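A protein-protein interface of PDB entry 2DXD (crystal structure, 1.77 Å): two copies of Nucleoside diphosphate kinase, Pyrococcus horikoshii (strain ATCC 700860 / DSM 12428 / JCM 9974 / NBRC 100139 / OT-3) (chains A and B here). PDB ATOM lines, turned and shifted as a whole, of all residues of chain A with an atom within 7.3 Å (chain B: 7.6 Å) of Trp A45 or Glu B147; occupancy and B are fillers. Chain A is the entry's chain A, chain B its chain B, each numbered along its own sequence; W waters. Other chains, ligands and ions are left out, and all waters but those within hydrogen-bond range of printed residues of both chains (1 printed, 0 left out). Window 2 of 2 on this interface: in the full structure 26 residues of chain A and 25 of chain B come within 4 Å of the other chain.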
ATOM      1  N   PRO A  16     -14.465   7.806   8.599  1.00  0.00           N
ATOM      2  CA  PRO A  16     -14.625   6.358   8.756  1.00  0.00           C
ATOM      3  C   PRO A  16     -13.395   5.518   8.431  1.00  0.00           C
ATOM      4  O   PRO A  16     -13.112   4.545   9.135  1.00  0.00           O
ATOM      5  CB  PRO A  16     -15.813   6.046   7.852  1.00  0.00           C
ATOM      6  CG  PRO A  16     -16.658   7.271   8.010  1.00  0.00           C
ATOM      7  CD  PRO A  16     -15.613   8.372   7.870  1.00  0.00           C
ATOM      8  N   LYS A  42     -16.180  14.258  20.206  1.00  0.00           N
ATOM      9  CA  LYS A  42     -17.120  13.178  20.461  1.00  0.00           C
ATOM     10  C   LYS A  42     -17.236  12.244  19.277  1.00  0.00           C
ATOM     11  O   LYS A  42     -17.073  12.657  18.128  1.00  0.00           O
ATOM     12  CB  LYS A  42     -18.507  13.738  20.796  1.00  0.00           C
ATOM     13  CG  LYS A  42     -19.122  14.616  19.718  1.00  0.00           C
ATOM     14  CD  LYS A  42     -20.475  15.154  20.175  1.00  0.00           C
ATOM     15  CE  LYS A  42     -21.055  16.140  19.179  1.00  0.00           C
ATOM     16  NZ  LYS A  42     -22.377  16.661  19.631  1.00  0.00           N
ATOM     17  N   MET A  43     -17.490  10.973  19.570  1.00  0.00           N
ATOM     18  CA  MET A  43     -17.690   9.986  18.526  1.00  0.00           C
ATOM     19  C   MET A  43     -19.190   9.964  18.270  1.00  0.00           C
ATOM     20  O   MET A  43     -19.986   9.825  19.202  1.00  0.00           O
ATOM     21  CB  MET A  43     -17.231   8.596  18.976  1.00  0.00           C
ATOM     22  CG  MET A  43     -17.607   7.501  17.978  1.00  0.00           C
ATOM     23  SD  MET A  43     -16.963   5.868  18.380  1.00  0.00           S
ATOM     24  CE  MET A  43     -15.273   5.995  17.733  1.00  0.00           C
ATOM     25  N   ILE A  44     -19.568  10.130  17.007  1.00  0.00           N
ATOM     26  CA  ILE A  44     -20.970  10.119  16.613  1.00  0.00           C
ATOM     27  C   ILE A  44     -21.093   9.331  15.321  1.00  0.00           C
ATOM     28  O   ILE A  44     -20.094   9.042  14.669  1.00  0.00           O
ATOM     29  CB  ILE A  44     -21.505  11.550  16.346  1.00  0.00           C
ATOM     30  CG1 ILE A  44     -20.719  12.207  15.203  1.00  0.00           C
ATOM     31  CG2 ILE A  44     -21.425  12.385  17.617  1.00  0.00           C
ATOM     32  CD1 ILE A  44     -21.258  13.572  14.781  1.00  0.00           C
ATOM     33  N   TRP A  45     -22.316   8.957  14.964  1.00  0.00           N
ATOM     34  CA  TRP A  45     -22.523   8.255  13.708  1.00  0.00           C
ATOM     35  C   TRP A  45     -23.445   9.179  12.920  1.00  0.00           C
ATOM     36  O   TRP A  45     -24.639   9.278  13.202  1.00  0.00           O
ATOM     37  CB  TRP A  45     -23.185   6.890  13.919  1.00  0.00           C
ATOM     38  CG  TRP A  45     -22.960   5.954  12.752  1.00  0.00           C
ATOM     39  CD1 TRP A  45     -22.822   6.303  11.437  1.00  0.00           C
ATOM     40  CD2 TRP A  45     -22.860   4.523  12.798  1.00  0.00           C
ATOM     41  NE1 TRP A  45     -22.640   5.182  10.663  1.00  0.00           N
ATOM     42  CE2 TRP A  45     -22.660   4.076  11.472  1.00  0.00           C
ATOM     43  CE3 TRP A  45     -22.922   3.575  13.829  1.00  0.00           C
ATOM     44  CZ2 TRP A  45     -22.521   2.719  11.148  1.00  0.00           C
ATOM     45  CZ3 TRP A  45     -22.782   2.223  13.509  1.00  0.00           C
ATOM     46  CH2 TRP A  45     -22.584   1.812  12.179  1.00  0.00           C
ATOM     47  N   ILE A  46     -22.869   9.874  11.948  1.00  0.00           N
ATOM     48  CA  ILE A  46     -23.605  10.828  11.129  1.00  0.00           C
ATOM     49  C   ILE A  46     -24.631  10.165  10.214  1.00  0.00           C
ATOM     50  O   ILE A  46     -24.310   9.197   9.525  1.00  0.00           O
ATOM     51  CB  ILE A  46     -22.626  11.640  10.247  1.00  0.00           C
ATOM     52  CG1 ILE A  46     -21.603  12.359  11.131  1.00  0.00           C
ATOM     53  CG2 ILE A  46     -23.393  12.628   9.384  1.00  0.00           C
ATOM     54  CD1 ILE A  46     -20.483  13.031  10.352  1.00  0.00           C
ATOM     55  N   ASP A  47     -25.868  10.661  10.217  1.00  0.00           N
ATOM     56  CA  ASP A  47     -26.863  10.099   9.307  1.00  0.00           C
ATOM     57  C   ASP A  47     -26.841  10.931   8.027  1.00  0.00           C
ATOM     58  O   ASP A  47     -26.206  11.983   7.979  1.00  0.00           O
ATOM     59  CB  ASP A  47     -28.277  10.060   9.921  1.00  0.00           C
ATOM     60  CG  ASP A  47     -28.795  11.421  10.347  1.00  0.00           C
ATOM     61  OD1 ASP A  47     -28.388  12.454   9.777  1.00  0.00           O
ATOM     62  OD2 ASP A  47     -29.649  11.447  11.259  1.00  0.00           O
ATOM     63  N   ARG A  48     -27.516  10.463   6.983  1.00  0.00           N
ATOM     64  CA  ARG A  48     -27.500  11.182   5.717  1.00  0.00           C
ATOM     65  C   ARG A  48     -27.932  12.644   5.805  1.00  0.00           C
ATOM     66  O   ARG A  48     -27.331  13.505   5.166  1.00  0.00           O
ATOM     67  CB  ARG A  48     -28.343  10.434   4.674  1.00  0.00           C
ATOM     68  CG  ARG A  48     -27.858   9.002   4.424  1.00  0.00           C
ATOM     69  CD  ARG A  48     -28.487   8.395   3.177  1.00  0.00           C
ATOM     70  NE  ARG A  48     -27.877   8.885   1.941  1.00  0.00           N
ATOM     71  CZ  ARG A  48     -26.722   8.446   1.447  1.00  0.00           C
ATOM     72  NH1 ARG A  48     -26.039   7.500   2.080  1.00  0.00           N
ATOM     73  NH2 ARG A  48     -26.248   8.949   0.312  1.00  0.00           N
ATOM     74  N   LEU A  50     -27.681  14.837   8.324  1.00  0.00           N
ATOM     75  CA  LEU A  50     -26.626  15.653   8.914  1.00  0.00           C
ATOM     76  C   LEU A  50     -25.449  15.770   7.948  1.00  0.00           C
ATOM     77  O   LEU A  50     -24.867  16.841   7.788  1.00  0.00           O
ATOM     78  CB  LEU A  50     -26.168  15.037  10.240  1.00  0.00           C
ATOM     79  CG  LEU A  50     -25.049  15.742  11.015  1.00  0.00           C
ATOM     80  CD1 LEU A  50     -25.407  17.204  11.261  1.00  0.00           C
ATOM     81  CD2 LEU A  50     -24.830  15.018  12.339  1.00  0.00           C
ATOM     82  N   ILE A  71     -18.882   9.306   4.367  1.00  0.00           N
ATOM     83  CA  ILE A  71     -18.863   9.937   5.682  1.00  0.00           C
ATOM     84  C   ILE A  71     -19.841   9.331   6.691  1.00  0.00           C
ATOM     85  O   ILE A  71     -19.703   9.547   7.898  1.00  0.00           O
ATOM     86  CB  ILE A  71     -19.111  11.466   5.556  1.00  0.00           C
ATOM     87  CG1 ILE A  71     -18.592  12.186   6.801  1.00  0.00           C
ATOM     88  CG2 ILE A  71     -20.583  11.752   5.351  1.00  0.00           C
ATOM     89  CD1 ILE A  71     -17.086  12.130   6.947  1.00  0.00           C
ATOM     90  N   THR A  72     -20.814   8.564   6.203  1.00  0.00           N
ATOM     91  CA  THR A  72     -21.799   7.926   7.079  1.00  0.00           C
ATOM     92  C   THR A  72     -21.585   6.416   7.195  1.00  0.00           C
ATOM     93  O   THR A  72     -22.395   5.717   7.807  1.00  0.00           O
ATOM     94  CB  THR A  72     -23.243   8.142   6.564  1.00  0.00           C
ATOM     95  OG1 THR A  72     -23.379   7.540   5.268  1.00  0.00           O
ATOM     96  CG2 THR A  72     -23.568   9.624   6.474  1.00  0.00           C
ATOM     97  N   LYS A  73     -20.491   5.917   6.625  1.00  0.00           N
ATOM     98  CA  LYS A  73     -20.207   4.482   6.631  1.00  0.00           C
ATOM     99  C   LYS A  73     -20.058   3.859   8.024  1.00  0.00           C
ATOM    100  O   LYS A  73     -20.569   2.762   8.278  1.00  0.00           O
ATOM    101  CB  LYS A  73     -18.958   4.206   5.790  1.00  0.00           C
ATOM    102  CG  LYS A  73     -18.755   2.744   5.431  1.00  0.00           C
ATOM    103  CD  LYS A  73     -17.618   2.589   4.431  1.00  0.00           C
ATOM    104  CE  LYS A  73     -17.424   1.135   4.031  1.00  0.00           C
ATOM    105  NZ  LYS A  73     -18.642   0.587   3.377  1.00  0.00           N
ATOM    106  N   THR A  74     -19.353   4.551   8.914  1.00  0.00           N
ATOM    107  CA  THR A  74     -19.151   4.088  10.287  1.00  0.00           C
ATOM    108  C   THR A  74     -19.109   5.330  11.171  1.00  0.00           C
ATOM    109  O   THR A  74     -19.200   6.457  10.674  1.00  0.00           O
ATOM    110  CB  THR A  74     -17.790   3.372  10.476  1.00  0.00           C
ATOM    111  OG1 THR A  74     -16.735   4.348  10.463  1.00  0.00           O
ATOM    112  CG2 THR A  74     -17.548   2.355   9.368  1.00  0.00           C
ATOM    113  N   PRO A  75     -18.998   5.145  12.497  1.00  0.00           N
ATOM    114  CA  PRO A  75     -18.940   6.336  13.343  1.00  0.00           C
ATOM    115  C   PRO A  75     -17.669   7.109  13.003  1.00  0.00           C
ATOM    116  O   PRO A  75     -16.719   6.552  12.445  1.00  0.00           O
ATOM    117  CB  PRO A  75     -18.874   5.756  14.754  1.00  0.00           C
ATOM    118  CG  PRO A  75     -19.685   4.501  14.632  1.00  0.00           C
ATOM    119  CD  PRO A  75     -19.207   3.930  13.310  1.00  0.00           C
ATOM    120  N   VAL A  76     -17.664   8.391  13.337  1.00  0.00           N
ATOM    121  CA  VAL A  76     -16.512   9.250  13.107  1.00  0.00           C
ATOM    122  C   VAL A  76     -16.250   9.978  14.413  1.00  0.00           C
ATOM    123  O   VAL A  76     -17.025   9.868  15.361  1.00  0.00           O
ATOM    124  CB  VAL A  76     -16.798  10.321  12.025  1.00  0.00           C
ATOM    125  CG1 VAL A  76     -17.093   9.660  10.691  1.00  0.00           C
ATOM    126  CG2 VAL A  76     -17.977  11.193  12.456  1.00  0.00           C
ATOM    127  N   ARG B   9     -17.227  -4.577  27.709  1.00  0.00           N
ATOM    128  CA  ARG B   9     -17.081  -3.143  27.517  1.00  0.00           C
ATOM    129  C   ARG B   9     -16.630  -2.583  28.854  1.00  0.00           C
ATOM    130  O   ARG B   9     -17.124  -2.995  29.906  1.00  0.00           O
ATOM    131  CB  ARG B   9     -18.408  -2.495  27.120  1.00  0.00           C
ATOM    132  CG  ARG B   9     -18.823  -2.732  25.677  1.00  0.00           C
ATOM    133  CD  ARG B   9     -20.113  -1.986  25.368  1.00  0.00           C
ATOM    134  NE  ARG B   9     -20.456  -2.044  23.950  1.00  0.00           N
ATOM    135  CZ  ARG B   9     -21.518  -1.454  23.415  1.00  0.00           C
ATOM    136  NH1 ARG B   9     -22.350  -0.758  24.181  1.00  0.00           N
ATOM    137  NH2 ARG B   9     -21.747  -1.552  22.114  1.00  0.00           N
ATOM    138  N   LYS B  37     -11.755  -1.776  20.611  1.00  0.00           N
ATOM    139  CA  LYS B  37     -12.586  -0.907  19.794  1.00  0.00           C
ATOM    140  C   LYS B  37     -13.227   0.200  20.617  1.00  0.00           C
ATOM    141  O   LYS B  37     -13.784  -0.053  21.682  1.00  0.00           O
ATOM    142  CB  LYS B  37     -13.681  -1.735  19.112  1.00  0.00           C
ATOM    143  CG  LYS B  37     -14.639  -0.934  18.233  1.00  0.00           C
ATOM    144  CD  LYS B  37     -15.757  -1.825  17.691  1.00  0.00           C
ATOM    145  CE  LYS B  37     -15.209  -2.938  16.808  1.00  0.00           C
ATOM    146  NZ  LYS B  37     -16.262  -3.935  16.443  1.00  0.00           N
ATOM    147  N   ILE B  38     -13.133   1.430  20.126  1.00  0.00           N
ATOM    148  CA  ILE B  38     -13.743   2.563  20.813  1.00  0.00           C
ATOM    149  C   ILE B  38     -15.194   2.608  20.337  1.00  0.00           C
ATOM    150  O   ILE B  38     -15.460   2.888  19.169  1.00  0.00           O
ATOM    151  CB  ILE B  38     -13.048   3.882  20.436  1.00  0.00           C
ATOM    152  CG1 ILE B  38     -11.569   3.810  20.822  1.00  0.00           C
ATOM    153  CG2 ILE B  38     -13.741   5.050  21.130  1.00  0.00           C
ATOM    154  CD1 ILE B  38     -10.739   4.971  20.302  1.00  0.00           C
ATOM    155  N   VAL B  39     -16.133   2.311  21.231  1.00  0.00           N
ATOM    156  CA  VAL B  39     -17.540   2.316  20.843  1.00  0.00           C
ATOM    157  C   VAL B  39     -18.285   3.556  21.322  1.00  0.00           C
ATOM    158  O   VAL B  39     -19.462   3.745  21.015  1.00  0.00           O
ATOM    159  CB  VAL B  39     -18.262   1.052  21.351  1.00  0.00           C
ATOM    160  CG1 VAL B  39     -17.638  -0.176  20.707  1.00  0.00           C
ATOM    161  CG2 VAL B  39     -18.176   0.963  22.870  1.00  0.00           C
ATOM    162  N   GLU B  82     -14.307  -1.715  23.837  1.00  0.00           N
ATOM    163  CA  GLU B  82     -14.930  -3.022  23.704  1.00  0.00           C
ATOM    164  C   GLU B  82     -13.938  -4.040  23.167  1.00  0.00           C
ATOM    165  O   GLU B  82     -13.164  -3.747  22.256  1.00  0.00           O
ATOM    166  CB  GLU B  82     -16.129  -2.919  22.759  1.00  0.00           C
ATOM    167  CG  GLU B  82     -16.921  -4.203  22.590  1.00  0.00           C
ATOM    168  CD  GLU B  82     -18.159  -3.998  21.736  1.00  0.00           C
ATOM    169  OE1 GLU B  82     -18.018  -3.815  20.510  1.00  0.00           O
ATOM    170  OE2 GLU B  82     -19.273  -4.007  22.294  1.00  0.00           O
ATOM    171  N   GLU B 143     -27.686   5.757  22.872  1.00  0.00           N
ATOM    172  CA  GLU B 143     -27.531   6.349  21.547  1.00  0.00           C
ATOM    173  C   GLU B 143     -26.121   6.869  21.280  1.00  0.00           C
ATOM    174  O   GLU B 143     -25.802   7.256  20.157  1.00  0.00           O
ATOM    175  CB  GLU B 143     -28.537   7.485  21.362  1.00  0.00           C
ATOM    176  CG  GLU B 143     -28.333   8.653  22.316  1.00  0.00           C
ATOM    177  CD  GLU B 143     -29.491   9.631  22.293  1.00  0.00           C
ATOM    178  OE1 GLU B 143     -30.611   9.231  22.676  1.00  0.00           O
ATOM    179  OE2 GLU B 143     -29.283  10.796  21.893  1.00  0.00           O
ATOM    180  N   GLU B 144     -25.285   6.873  22.315  1.00  0.00           N
ATOM    181  CA  GLU B 144     -23.909   7.351  22.200  1.00  0.00           C
ATOM    182  C   GLU B 144     -22.898   6.212  22.054  1.00  0.00           C
ATOM    183  O   GLU B 144     -21.695   6.457  21.949  1.00  0.00           O
ATOM    184  CB  GLU B 144     -23.546   8.190  23.427  1.00  0.00           C
ATOM    185  CG  GLU B 144     -24.296   9.508  23.529  1.00  0.00           C
ATOM    186  CD  GLU B 144     -23.981  10.257  24.810  1.00  0.00           C
ATOM    187  OE1 GLU B 144     -24.464   9.841  25.883  1.00  0.00           O
ATOM    188  OE2 GLU B 144     -23.244  11.262  24.745  1.00  0.00           O
ATOM    189  N   LEU B 145     -23.390   4.977  22.059  1.00  0.00           N
ATOM    190  CA  LEU B 145     -22.540   3.794  21.930  1.00  0.00           C
ATOM    191  C   LEU B 145     -22.862   3.133  20.594  1.00  0.00           C
ATOM    192  O   LEU B 145     -24.029   3.000  20.227  1.00  0.00           O
ATOM    193  CB  LEU B 145     -22.801   2.841  23.095  1.00  0.00           C
ATOM    194  CG  LEU B 145     -22.621   3.516  24.460  1.00  0.00           C
ATOM    195  CD1 LEU B 145     -23.047   2.570  25.566  1.00  0.00           C
ATOM    196  CD2 LEU B 145     -21.167   3.941  24.637  1.00  0.00           C
ATOM    197  N   PHE B 146     -21.833   2.697  19.878  1.00  0.00           N
ATOM    198  CA  PHE B 146     -22.042   2.133  18.551  1.00  0.00           C
ATOM    199  C   PHE B 146     -21.487   0.742  18.285  1.00  0.00           C
ATOM    200  O   PHE B 146     -20.530   0.299  18.918  1.00  0.00           O
ATOM    201  CB  PHE B 146     -21.456   3.100  17.518  1.00  0.00           C
ATOM    202  CG  PHE B 146     -21.851   4.533  17.742  1.00  0.00           C
ATOM    203  CD1 PHE B 146     -23.118   4.981  17.388  1.00  0.00           C
ATOM    204  CD2 PHE B 146     -20.965   5.426  18.339  1.00  0.00           C
ATOM    205  CE1 PHE B 146     -23.499   6.300  17.626  1.00  0.00           C
ATOM    206  CE2 PHE B 146     -21.335   6.749  18.582  1.00  0.00           C
ATOM    207  CZ  PHE B 146     -22.606   7.186  18.225  1.00  0.00           C
ATOM    208  N   GLU B 147     -22.112   0.069  17.325  1.00  0.00           N
ATOM    209  CA  GLU B 147     -21.694  -1.256  16.897  1.00  0.00           C
ATOM    210  C   GLU B 147     -21.274  -1.082  15.445  1.00  0.00           C
ATOM    211  O   GLU B 147     -22.099  -0.763  14.586  1.00  0.00           O
ATOM    212  CB  GLU B 147     -22.854  -2.250  16.999  1.00  0.00           C
ATOM    213  CG  GLU B 147     -23.289  -2.532  18.428  1.00  0.00           C
ATOM    214  CD  GLU B 147     -24.443  -3.510  18.506  1.00  0.00           C
ATOM    215  OE1 GLU B 147     -24.306  -4.636  17.981  1.00  0.00           O
ATOM    216  OE2 GLU B 147     -25.487  -3.153  19.094  1.00  0.00           O
ATOM    217  N   TYR B 148     -19.989  -1.270  15.177  1.00  0.00           N
ATOM    218  CA  TYR B 148     -19.473  -1.109  13.827  1.00  0.00           C
ATOM    219  C   TYR B 148     -18.208  -1.936  13.673  1.00  0.00           C
ATOM    220  O   TYR B 148     -17.580  -2.324  14.657  1.00  0.00           O
ATOM    221  CB  TYR B 148     -19.167   0.364  13.561  1.00  0.00           C
ATOM    222  CG  TYR B 148     -18.013   0.887  14.379  1.00  0.00           C
ATOM    223  CD1 TYR B 148     -16.718   0.907  13.860  1.00  0.00           C
ATOM    224  CD2 TYR B 148     -18.207   1.332  15.686  1.00  0.00           C
ATOM    225  CE1 TYR B 148     -15.645   1.358  14.621  1.00  0.00           C
ATOM    226  CE2 TYR B 148     -17.138   1.786  16.458  1.00  0.00           C
ATOM    227  CZ  TYR B 148     -15.861   1.796  15.917  1.00  0.00           C
ATOM    228  OH  TYR B 148     -14.802   2.260  16.664  1.00  0.00           O
ATOM    229  N   PRO B 149     -17.805  -2.205  12.429  1.00  0.00           N
ATOM    230  CA  PRO B 149     -16.599  -3.000  12.208  1.00  0.00           C
ATOM    231  C   PRO B 149     -15.276  -2.243  12.193  1.00  0.00           C
ATOM    232  O   PRO B 149     -15.157  -1.178  11.581  1.00  0.00           O
ATOM    233  CB  PRO B 149     -16.877  -3.652  10.861  1.00  0.00           C
ATOM    234  CG  PRO B 149     -17.581  -2.548  10.126  1.00  0.00           C
ATOM    235  CD  PRO B 149     -18.554  -2.019  11.170  1.00  0.00           C
HETATM  236  O   HOH W   1     -19.869   8.476  21.793  1.00  0.00           O
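The side-chain sulfur of Met A43 lies close to the backbone carbonyl oxygen of Ile B38 (3.4 Å).
The side-chain hydroxyl of Tyr B148 is in hydrogen-bond range of the backbone carbonyl oxygen of Ile B38 (2.7 Å).
The side-chain amino group (NZ) of Lys B37 sits at hydrogen-bond distance from the backbone carbonyl oxygen (O) of Tyr B148 (2.7 Å).
The indole nitrogen of Trp A45 is in hydrogen-bond range of the backbone carbonyl oxygen of Thr A72 (2.9 Å).
The backbone carbonyl oxygen of Ile A44 sits at hydrogen-bond distance from the backbone NH of Val A76, at 2.8 Å.
The backbone carbonyl oxygen (O) of Val B39 lies within hydrogen-bond range of the backbone NH (N) of Phe B146 (2.8 Å).
Met A43 touches Val B39.
Met A43 touches Phe B146 (O to CE2, 3.4 Å).
Met A43 touches Tyr B148 (CE to OH, 3.9 Å).
Ile A44 touches Phe B146 (CA to CZ, 3.7 Å).
Trp A45 touches Phe B146 (N to CZ, 3.7 Å).
CZ3 of Trp A45 touches O of Glu B147 (3.2 Å).
Trp A45 touches Tyr B148.
Phe B146 touches Pro A75 (CB to CG, 3.7 Å).
Pro A75 touches Tyr B148 (CD to CG, 3.4 Å).
Trp A45 touches just these residues of chain B: Phe B146 (3.7 Å), Glu B147 (3.2 Å) and Tyr B148 (3.96 Å).
Glu B147 touches just one residue of chain A: Trp A45.
Printed residues of chain A within 4 Å of Phe B146: Met A43 (3.4 Å), Ile A44 (3.7 Å), Trp A45 (3.7 Å) and Pro A75 (3.7 Å).
Of the printed residues of chain B, Met A43 touches Ile B38, Val B39, Phe B146 and Tyr B148.
Of the printed residues of chain B, Pro A75 touches Phe B146 and Tyr B148.
The nearest residue of chain A that does not touch Glu B147 is Pro A75 (5.7 Å).
The nearest printed residue of chain B that does not touch Met A43 is Glu B144 (4.7 Å).
Printed residues of chain B that touch a printed residue of chain A: Ile B38, Val B39, Phe B146, Glu B147 and Tyr B148.
Of the 15 printed residues of chain A, 4 touch a printed residue of chain B.
Among the printed residues, no Asp or Glu carboxylate lies within 4 Å of a Lys or Arg side-chain nitrogen of the other chain.
No position is printed for both chains.
Of the 10 pairs that touch across the chains among the printed residues, none has its exchanged pair printed and touching as well.
Water W1 bridges O of Glu B144 (2.7 Å) and O of Met A43 (2.9 Å).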
